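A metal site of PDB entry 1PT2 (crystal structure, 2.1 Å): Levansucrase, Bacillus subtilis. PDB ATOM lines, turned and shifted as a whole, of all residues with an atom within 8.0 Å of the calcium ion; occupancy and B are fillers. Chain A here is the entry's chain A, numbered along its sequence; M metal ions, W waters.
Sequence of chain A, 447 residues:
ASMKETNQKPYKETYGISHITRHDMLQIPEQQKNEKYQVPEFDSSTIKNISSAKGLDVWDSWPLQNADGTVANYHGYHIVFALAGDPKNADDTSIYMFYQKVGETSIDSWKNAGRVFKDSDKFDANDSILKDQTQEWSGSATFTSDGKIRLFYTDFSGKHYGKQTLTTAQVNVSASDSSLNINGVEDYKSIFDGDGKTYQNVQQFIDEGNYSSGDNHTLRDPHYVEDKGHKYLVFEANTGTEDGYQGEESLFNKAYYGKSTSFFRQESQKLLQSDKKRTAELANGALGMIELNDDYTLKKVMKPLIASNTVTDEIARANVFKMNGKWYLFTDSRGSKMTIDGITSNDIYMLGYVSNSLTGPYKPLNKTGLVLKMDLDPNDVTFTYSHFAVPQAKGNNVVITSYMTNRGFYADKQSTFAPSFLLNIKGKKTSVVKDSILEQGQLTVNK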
ATOM      1  N   GLN A 200      -6.871 -36.535  12.207  1.00  0.00           N
ATOM      2  CA  GLN A 200      -7.659 -35.345  11.902  1.00  0.00           C
ATOM      3  C   GLN A 200      -8.169 -35.386  10.472  1.00  0.00           C
ATOM      4  O   GLN A 200      -7.461 -35.844   9.565  1.00  0.00           O
ATOM      5  CB  GLN A 200      -6.789 -34.084  12.107  1.00  0.00           C
ATOM      6  CG  GLN A 200      -7.571 -32.768  12.202  1.00  0.00           C
ATOM      7  CD  GLN A 200      -6.663 -31.535  12.139  1.00  0.00           C
ATOM      8  OE1 GLN A 200      -5.769 -31.449  11.292  1.00  0.00           O
ATOM      9  NE2 GLN A 200      -6.892 -30.591  13.042  1.00  0.00           N
ATOM     10  N   PHE A 205     -10.394 -29.233  10.711  1.00  0.00           N
ATOM     11  CA  PHE A 205      -9.613 -28.067  10.306  1.00  0.00           C
ATOM     12  C   PHE A 205     -10.535 -26.861  10.108  1.00  0.00           C
ATOM     13  O   PHE A 205     -10.228 -25.754  10.550  1.00  0.00           O
ATOM     14  CB  PHE A 205      -8.879 -28.379   9.000  1.00  0.00           C
ATOM     15  CG  PHE A 205      -8.004 -27.278   8.493  1.00  0.00           C
ATOM     16  CD1 PHE A 205      -7.057 -26.676   9.311  1.00  0.00           C
ATOM     17  CD2 PHE A 205      -8.112 -26.846   7.165  1.00  0.00           C
ATOM     18  CE1 PHE A 205      -6.237 -25.660   8.824  1.00  0.00           C
ATOM     19  CE2 PHE A 205      -7.283 -25.834   6.676  1.00  0.00           C
ATOM     20  CZ  PHE A 205      -6.346 -25.233   7.509  1.00  0.00           C
ATOM     21  N   GLU A 208     -11.888 -25.157  13.269  1.00  0.00           N
ATOM     22  CA  GLU A 208     -10.955 -24.191  13.872  1.00  0.00           C
ATOM     23  C   GLU A 208     -10.953 -22.804  13.184  1.00  0.00           C
ATOM     24  O   GLU A 208     -10.435 -21.839  13.745  1.00  0.00           O
ATOM     25  CB  GLU A 208      -9.508 -24.731  13.847  1.00  0.00           C
ATOM     26  CG  GLU A 208      -9.279 -26.106  14.485  1.00  0.00           C
ATOM     27  CD  GLU A 208      -9.252 -26.106  16.006  1.00  0.00           C
ATOM     28  OE1 GLU A 208      -9.279 -25.014  16.623  1.00  0.00           O
ATOM     29  OE2 GLU A 208      -9.207 -27.211  16.600  1.00  0.00           O
ATOM     30  N   SER A 213      -6.793 -19.842  11.453  1.00  0.00           N
ATOM     31  CA  SER A 213      -6.583 -20.316  12.823  1.00  0.00           C
ATOM     32  C   SER A 213      -5.103 -20.552  13.173  1.00  0.00           C
ATOM     33  O   SER A 213      -4.762 -20.556  14.346  1.00  0.00           O
ATOM     34  CB  SER A 213      -7.382 -21.616  13.041  1.00  0.00           C
ATOM     35  OG  SER A 213      -6.781 -22.702  12.377  1.00  0.00           O
ATOM     36  N   GLY A 214      -4.254 -20.741  12.165  1.00  0.00           N
ATOM     37  CA  GLY A 214      -2.876 -21.155  12.380  1.00  0.00           C
ATOM     38  C   GLY A 214      -2.672 -22.671  12.398  1.00  0.00           C
ATOM     39  O   GLY A 214      -1.545 -23.156  12.480  1.00  0.00           O
ATOM     40  N   ASP A 215      -3.766 -23.422  12.328  1.00  0.00           N
ATOM     41  CA  ASP A 215      -3.674 -24.882  12.326  1.00  0.00           C
ATOM     42  C   ASP A 215      -3.107 -25.340  10.997  1.00  0.00           C
ATOM     43  O   ASP A 215      -3.245 -24.656   9.993  1.00  0.00           O
ATOM     44  CB  ASP A 215      -5.050 -25.523  12.585  1.00  0.00           C
ATOM     45  CG  ASP A 215      -4.951 -26.968  13.057  1.00  0.00           C
ATOM     46  OD1 ASP A 215      -3.858 -27.416  13.457  1.00  0.00           O
ATOM     47  OD2 ASP A 215      -5.941 -27.731  13.074  1.00  0.00           O
ATOM     48  N   ASN A 216      -2.421 -26.485  10.998  1.00  0.00           N
ATOM     49  CA  ASN A 216      -1.866 -27.044   9.778  1.00  0.00           C
ATOM     50  C   ASN A 216      -2.366 -28.471   9.622  1.00  0.00           C
ATOM     51  O   ASN A 216      -1.848 -29.399  10.233  1.00  0.00           O
ATOM     52  CB  ASN A 216      -0.335 -27.016   9.808  1.00  0.00           C
ATOM     53  CG  ASN A 216       0.301 -27.506   8.508  1.00  0.00           C
ATOM     54  OD1 ASN A 216      -0.391 -27.763   7.529  1.00  0.00           O
ATOM     55  ND2 ASN A 216       1.630 -27.644   8.512  1.00  0.00           N
ATOM     56  N   HIS A 217      -3.380 -28.623   8.779  1.00  0.00           N
ATOM     57  CA  HIS A 217      -3.981 -29.926   8.525  1.00  0.00           C
ATOM     58  C   HIS A 217      -3.222 -30.666   7.438  1.00  0.00           C
ATOM     59  O   HIS A 217      -3.006 -30.145   6.334  1.00  0.00           O
ATOM     60  CB  HIS A 217      -5.451 -29.799   8.125  1.00  0.00           C
ATOM     61  CG  HIS A 217      -6.059 -31.105   7.722  1.00  0.00           C
ATOM     62  ND1 HIS A 217      -6.253 -32.135   8.608  1.00  0.00           N
ATOM     63  CD2 HIS A 217      -6.475 -31.557   6.514  1.00  0.00           C
ATOM     64  CE1 HIS A 217      -6.786 -33.162   7.971  1.00  0.00           C
ATOM     65  NE2 HIS A 217      -6.932 -32.839   6.708  1.00  0.00           N
ATOM     66  N   THR A 218      -2.828 -31.885   7.768  1.00  0.00           N
ATOM     67  CA  THR A 218      -2.090 -32.743   6.851  1.00  0.00           C
ATOM     68  C   THR A 218      -2.708 -34.142   6.848  1.00  0.00           C
ATOM     69  O   THR A 218      -3.172 -34.641   7.868  1.00  0.00           O
ATOM     70  CB  THR A 218      -0.595 -32.801   7.245  1.00  0.00           C
ATOM     71  OG1 THR A 218      -0.399 -33.673   8.368  1.00  0.00           O
ATOM     72  CG2 THR A 218      -0.069 -31.438   7.716  1.00  0.00           C
ATOM     73  N   ALA A 237       0.242 -37.276   9.038  1.00  0.00           N
ATOM     74  CA  ALA A 237      -1.100 -36.944   9.488  1.00  0.00           C
ATOM     75  C   ALA A 237      -1.025 -36.021  10.696  1.00  0.00           C
ATOM     76  O   ALA A 237       0.013 -35.429  10.994  1.00  0.00           O
ATOM     77  CB  ALA A 237      -1.884 -38.215   9.814  1.00  0.00           C
ATOM     78  N   ASN A 238      -2.166 -35.882  11.359  1.00  0.00           N
ATOM     79  CA  ASN A 238      -2.265 -35.213  12.642  1.00  0.00           C
ATOM     80  C   ASN A 238      -3.202 -36.047  13.502  1.00  0.00           C
ATOM     81  O   ASN A 238      -4.053 -36.745  12.972  1.00  0.00           O
ATOM     82  CB  ASN A 238      -2.799 -33.777  12.465  1.00  0.00           C
ATOM     83  CG  ASN A 238      -1.889 -32.913  11.617  1.00  0.00           C
ATOM     84  OD1 ASN A 238      -2.004 -32.899  10.385  1.00  0.00           O
ATOM     85  ND2 ASN A 238      -0.987 -32.180  12.252  1.00  0.00           N
ATOM     86  N   THR A 239      -3.041 -35.986  14.818  1.00  0.00           N
ATOM     87  CA  THR A 239      -3.855 -36.801  15.718  1.00  0.00           C
ATOM     88  C   THR A 239      -5.307 -36.349  15.671  1.00  0.00           C
ATOM     89  O   THR A 239      -5.611 -35.232  15.262  1.00  0.00           O
ATOM     90  CB  THR A 239      -3.350 -36.712  17.170  1.00  0.00           C
ATOM     91  OG1 THR A 239      -3.278 -35.346  17.568  1.00  0.00           O
ATOM     92  CG2 THR A 239      -1.918 -37.232  17.309  1.00  0.00           C
ATOM     93  N   TYR A 245      -5.307 -35.088  21.098  1.00  0.00           N
ATOM     94  CA  TYR A 245      -5.587 -34.046  20.132  1.00  0.00           C
ATOM     95  C   TYR A 245      -4.878 -32.734  20.499  1.00  0.00           C
ATOM     96  O   TYR A 245      -4.402 -32.562  21.621  1.00  0.00           O
ATOM     97  CB  TYR A 245      -7.106 -33.828  20.052  1.00  0.00           C
ATOM     98  CG  TYR A 245      -7.587 -33.146  18.785  1.00  0.00           C
ATOM     99  CD1 TYR A 245      -7.066 -33.486  17.539  1.00  0.00           C
ATOM    100  CD2 TYR A 245      -8.560 -32.162  18.841  1.00  0.00           C
ATOM    101  CE1 TYR A 245      -7.511 -32.859  16.373  1.00  0.00           C
ATOM    102  CE2 TYR A 245      -9.010 -31.521  17.673  1.00  0.00           C
ATOM    103  CZ  TYR A 245      -8.482 -31.879  16.451  1.00  0.00           C
ATOM    104  OH  TYR A 245      -8.913 -31.257  15.314  1.00  0.00           O
ATOM    105  N   GLN A 246      -4.795 -31.848  19.516  1.00  0.00           N
ATOM    106  CA  GLN A 246      -4.417 -30.455  19.735  1.00  0.00           C
ATOM    107  C   GLN A 246      -5.367 -29.779  20.742  1.00  0.00           C
ATOM    108  O   GLN A 246      -6.480 -30.244  20.950  1.00  0.00           O
ATOM    109  CB  GLN A 246      -4.433 -29.687  18.403  1.00  0.00           C
ATOM    110  CG  GLN A 246      -5.813 -29.544  17.759  1.00  0.00           C
ATOM    111  CD  GLN A 246      -5.756 -29.197  16.278  1.00  0.00           C
ATOM    112  OE1 GLN A 246      -4.790 -29.561  15.594  1.00  0.00           O
ATOM    113  NE2 GLN A 246      -6.783 -28.514  15.779  1.00  0.00           N
ATOM    114  N   GLY A 247      -4.899 -28.690  21.341  1.00  0.00           N
ATOM    115  CA  GLY A 247      -5.688 -27.908  22.275  1.00  0.00           C
ATOM    116  C   GLY A 247      -4.865 -27.402  23.447  1.00  0.00           C
ATOM    117  O   GLY A 247      -3.704 -27.803  23.647  1.00  0.00           O
ATOM    118  N   THR A 279       1.189 -21.965  18.980  1.00  0.00           N
ATOM    119  CA  THR A 279       1.771 -22.872  17.999  1.00  0.00           C
ATOM    120  C   THR A 279       1.853 -24.295  18.559  1.00  0.00           C
ATOM    121  O   THR A 279       1.484 -25.263  17.881  1.00  0.00           O
ATOM    122  CB  THR A 279       3.175 -22.380  17.596  1.00  0.00           C
ATOM    123  OG1 THR A 279       3.087 -21.072  17.037  1.00  0.00           O
ATOM    124  CG2 THR A 279       3.746 -23.209  16.456  1.00  0.00           C
ATOM    125  N   ALA A 280       2.324 -24.401  19.802  1.00  0.00           N
ATOM    126  CA  ALA A 280       2.479 -25.691  20.475  1.00  0.00           C
ATOM    127  C   ALA A 280       1.128 -26.364  20.712  1.00  0.00           C
ATOM    128  O   ALA A 280       1.008 -27.577  20.584  1.00  0.00           O
ATOM    129  CB  ALA A 280       3.225 -25.515  21.786  1.00  0.00           C
ATOM    130  N   GLU A 281       0.123 -25.559  21.058  1.00  0.00           N
ATOM    131  CA  GLU A 281      -1.227 -26.082  21.287  1.00  0.00           C
ATOM    132  C   GLU A 281      -1.779 -26.713  20.012  1.00  0.00           C
ATOM    133  O   GLU A 281      -2.370 -27.791  20.065  1.00  0.00           O
ATOM    134  CB  GLU A 281      -2.150 -24.963  21.814  1.00  0.00           C
ATOM    135  CG  GLU A 281      -1.847 -24.566  23.262  1.00  0.00           C
ATOM    136  CD  GLU A 281      -2.547 -23.295  23.724  1.00  0.00           C
ATOM    137  OE1 GLU A 281      -3.066 -22.522  22.893  1.00  0.00           O
ATOM    138  OE2 GLU A 281      -2.580 -23.073  24.954  1.00  0.00           O
ATOM    139  N   LEU A 282      -1.550 -26.073  18.871  1.00  0.00           N
ATOM    140  CA  LEU A 282      -2.031 -26.546  17.571  1.00  0.00           C
ATOM    141  C   LEU A 282      -1.196 -27.704  16.999  1.00  0.00           C
ATOM    142  O   LEU A 282      -1.653 -28.391  16.077  1.00  0.00           O
ATOM    143  CB  LEU A 282      -2.012 -25.408  16.552  1.00  0.00           C
ATOM    144  CG  LEU A 282      -2.968 -24.235  16.813  1.00  0.00           C
ATOM    145  CD1 LEU A 282      -2.464 -22.967  16.125  1.00  0.00           C
ATOM    146  CD2 LEU A 282      -4.369 -24.582  16.333  1.00  0.00           C
ATOM    147  N   ALA A 283       0.004 -27.898  17.522  1.00  0.00           N
ATOM    148  CA  ALA A 283       0.925 -28.897  16.996  1.00  0.00           C
ATOM    149  C   ALA A 283       0.551 -30.307  17.447  1.00  0.00           C
ATOM    150  O   ALA A 283       0.617 -30.619  18.625  1.00  0.00           O
ATOM    151  CB  ALA A 283       2.355 -28.563  17.425  1.00  0.00           C
ATOM    152  N   ASN A 284       0.128 -31.137  16.510  1.00  0.00           N
ATOM    153  CA  ASN A 284      -0.190 -32.526  16.827  1.00  0.00           C
ATOM    154  C   ASN A 284       0.078 -33.418  15.623  1.00  0.00           C
ATOM    155  O   ASN A 284      -0.739 -34.261  15.263  1.00  0.00           O
ATOM    156  CB  ASN A 284      -1.641 -32.652  17.310  1.00  0.00           C
ATOM    157  CG  ASN A 284      -2.645 -32.402  16.200  1.00  0.00           C
ATOM    158  OD1 ASN A 284      -2.376 -31.672  15.251  1.00  0.00           O
ATOM    159  ND2 ASN A 284      -3.825 -33.018  16.319  1.00  0.00           N
ATOM    160  N   GLY A 285       1.238 -33.226  15.004  1.00  0.00           N
ATOM    161  CA  GLY A 285       1.659 -34.065  13.897  1.00  0.00           C
ATOM    162  C   GLY A 285       1.756 -35.514  14.305  1.00  0.00           C
ATOM    163  O   GLY A 285       1.920 -35.836  15.485  1.00  0.00           O
ATOM    164  N   THR A 312       5.726 -29.881  16.805  1.00  0.00           N
ATOM    165  CA  THR A 312       5.388 -29.418  15.461  1.00  0.00           C
ATOM    166  C   THR A 312       4.110 -30.069  14.934  1.00  0.00           C
ATOM    167  O   THR A 312       3.715 -31.140  15.376  1.00  0.00           O
ATOM    168  CB  THR A 312       6.562 -29.656  14.474  1.00  0.00           C
ATOM    169  OG1 THR A 312       6.203 -29.235  13.149  1.00  0.00           O
ATOM    170  CG2 THR A 312       6.868 -31.138  14.327  1.00  0.00           C
ATOM    171  N   ASP A 313       3.474 -29.384  13.993  1.00  0.00           N
ATOM    172  CA  ASP A 313       2.264 -29.849  13.338  1.00  0.00           C
ATOM    173  C   ASP A 313       2.582 -30.574  12.027  1.00  0.00           C
ATOM    174  O   ASP A 313       1.666 -31.067  11.354  1.00  0.00           O
ATOM    175  CB  ASP A 313       1.364 -28.646  13.024  1.00  0.00           C
ATOM    176  CG  ASP A 313      -0.085 -28.896  13.333  1.00  0.00           C
ATOM    177  OD1 ASP A 313      -0.452 -30.013  13.756  1.00  0.00           O
ATOM    178  OD2 ASP A 313      -0.961 -28.016  13.176  1.00  0.00           O
ATOM    179  N   GLU A 314       3.864 -30.626  11.663  1.00  0.00           N
ATOM    180  CA  GLU A 314       4.258 -31.062  10.334  1.00  0.00           C
ATOM    181  C   GLU A 314       5.475 -31.965  10.346  1.00  0.00           C
ATOM    182  O   GLU A 314       6.617 -31.484  10.365  1.00  0.00           O
ATOM    183  CB  GLU A 314       4.517 -29.844   9.428  1.00  0.00           C
ATOM    184  CG  GLU A 314       4.625 -30.200   7.947  1.00  0.00           C
ATOM    185  CD  GLU A 314       4.862 -28.987   7.061  1.00  0.00           C
ATOM    186  OE1 GLU A 314       6.044 -28.683   6.776  1.00  0.00           O
ATOM    187  OE2 GLU A 314       3.867 -28.356   6.642  1.00  0.00           O
HETATM  188 CA    CA M   1      -2.805 -29.273  14.346  1.00  0.00          CA
HETATM  189  O   HOH W   1      -3.480 -30.372  12.280  1.00  0.00           O
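Water W1 lies within hydrogen-bond range of OE1 of Gln 200, O of Asn 216 and ND2 of Asn 238.
The calcium ion is bound by the backbone carbonyl oxygen (O) of Leu 282 (2.3 Å), the side-chain carboxylate (OD1) of Asp 215 (2.3 Å), the side-chain amide oxygen (OE1) of Gln 246 (2.4 Å), water W1 (2.4 Å), the side-chain carboxylate (OD2) of Asp 313 (2.5 Å), the side-chain carboxylate (OD1) of Asp 313 (2.5 Å) and the side-chain amide oxygen (OD1) of Asn 284 (2.6 Å). The calcium ion has seven donor atoms within binding distance.
NE2 of Gln 200 lies within hydrogen-bond range of OD2 of Asp 215 (3.0 Å). The backbone NH of Asp 215 lies within hydrogen-bond range of the side-chain hydroxyl of Ser 213, at 3.1 Å. The side-chain amide nitrogen (NE2) of Gln 200 lies close to the side-chain amide nitrogen (NE2) of Gln 246 (3.4 Å). The side-chain amide nitrogen (NE2) of Gln 246 lies within hydrogen-bond range of the side-chain carboxylate (OE2) of Glu 208 (2.9 Å). The backbone carbonyl oxygen (O) of Asp 313 lies within hydrogen-bond range of the side-chain amide nitrogen (ND2) of Asn 238 (3.0 Å). OD2 of Asp 313 sits close to N of Asn 216 (3.0 Å). The side-chain amide oxygen of Asn 284 sits close to the side-chain amide nitrogen of Asn 238, 3.3 Å away. ND2 of Asn 284 sits at hydrogen-bond distance from OG1 of Thr 239 (2.7 Å).
Of the 25 residues printed, 5 come within 4 Å of the calcium ion. Along chain A the residues within 4 Å of the calcium ion span positions 215 to 313.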
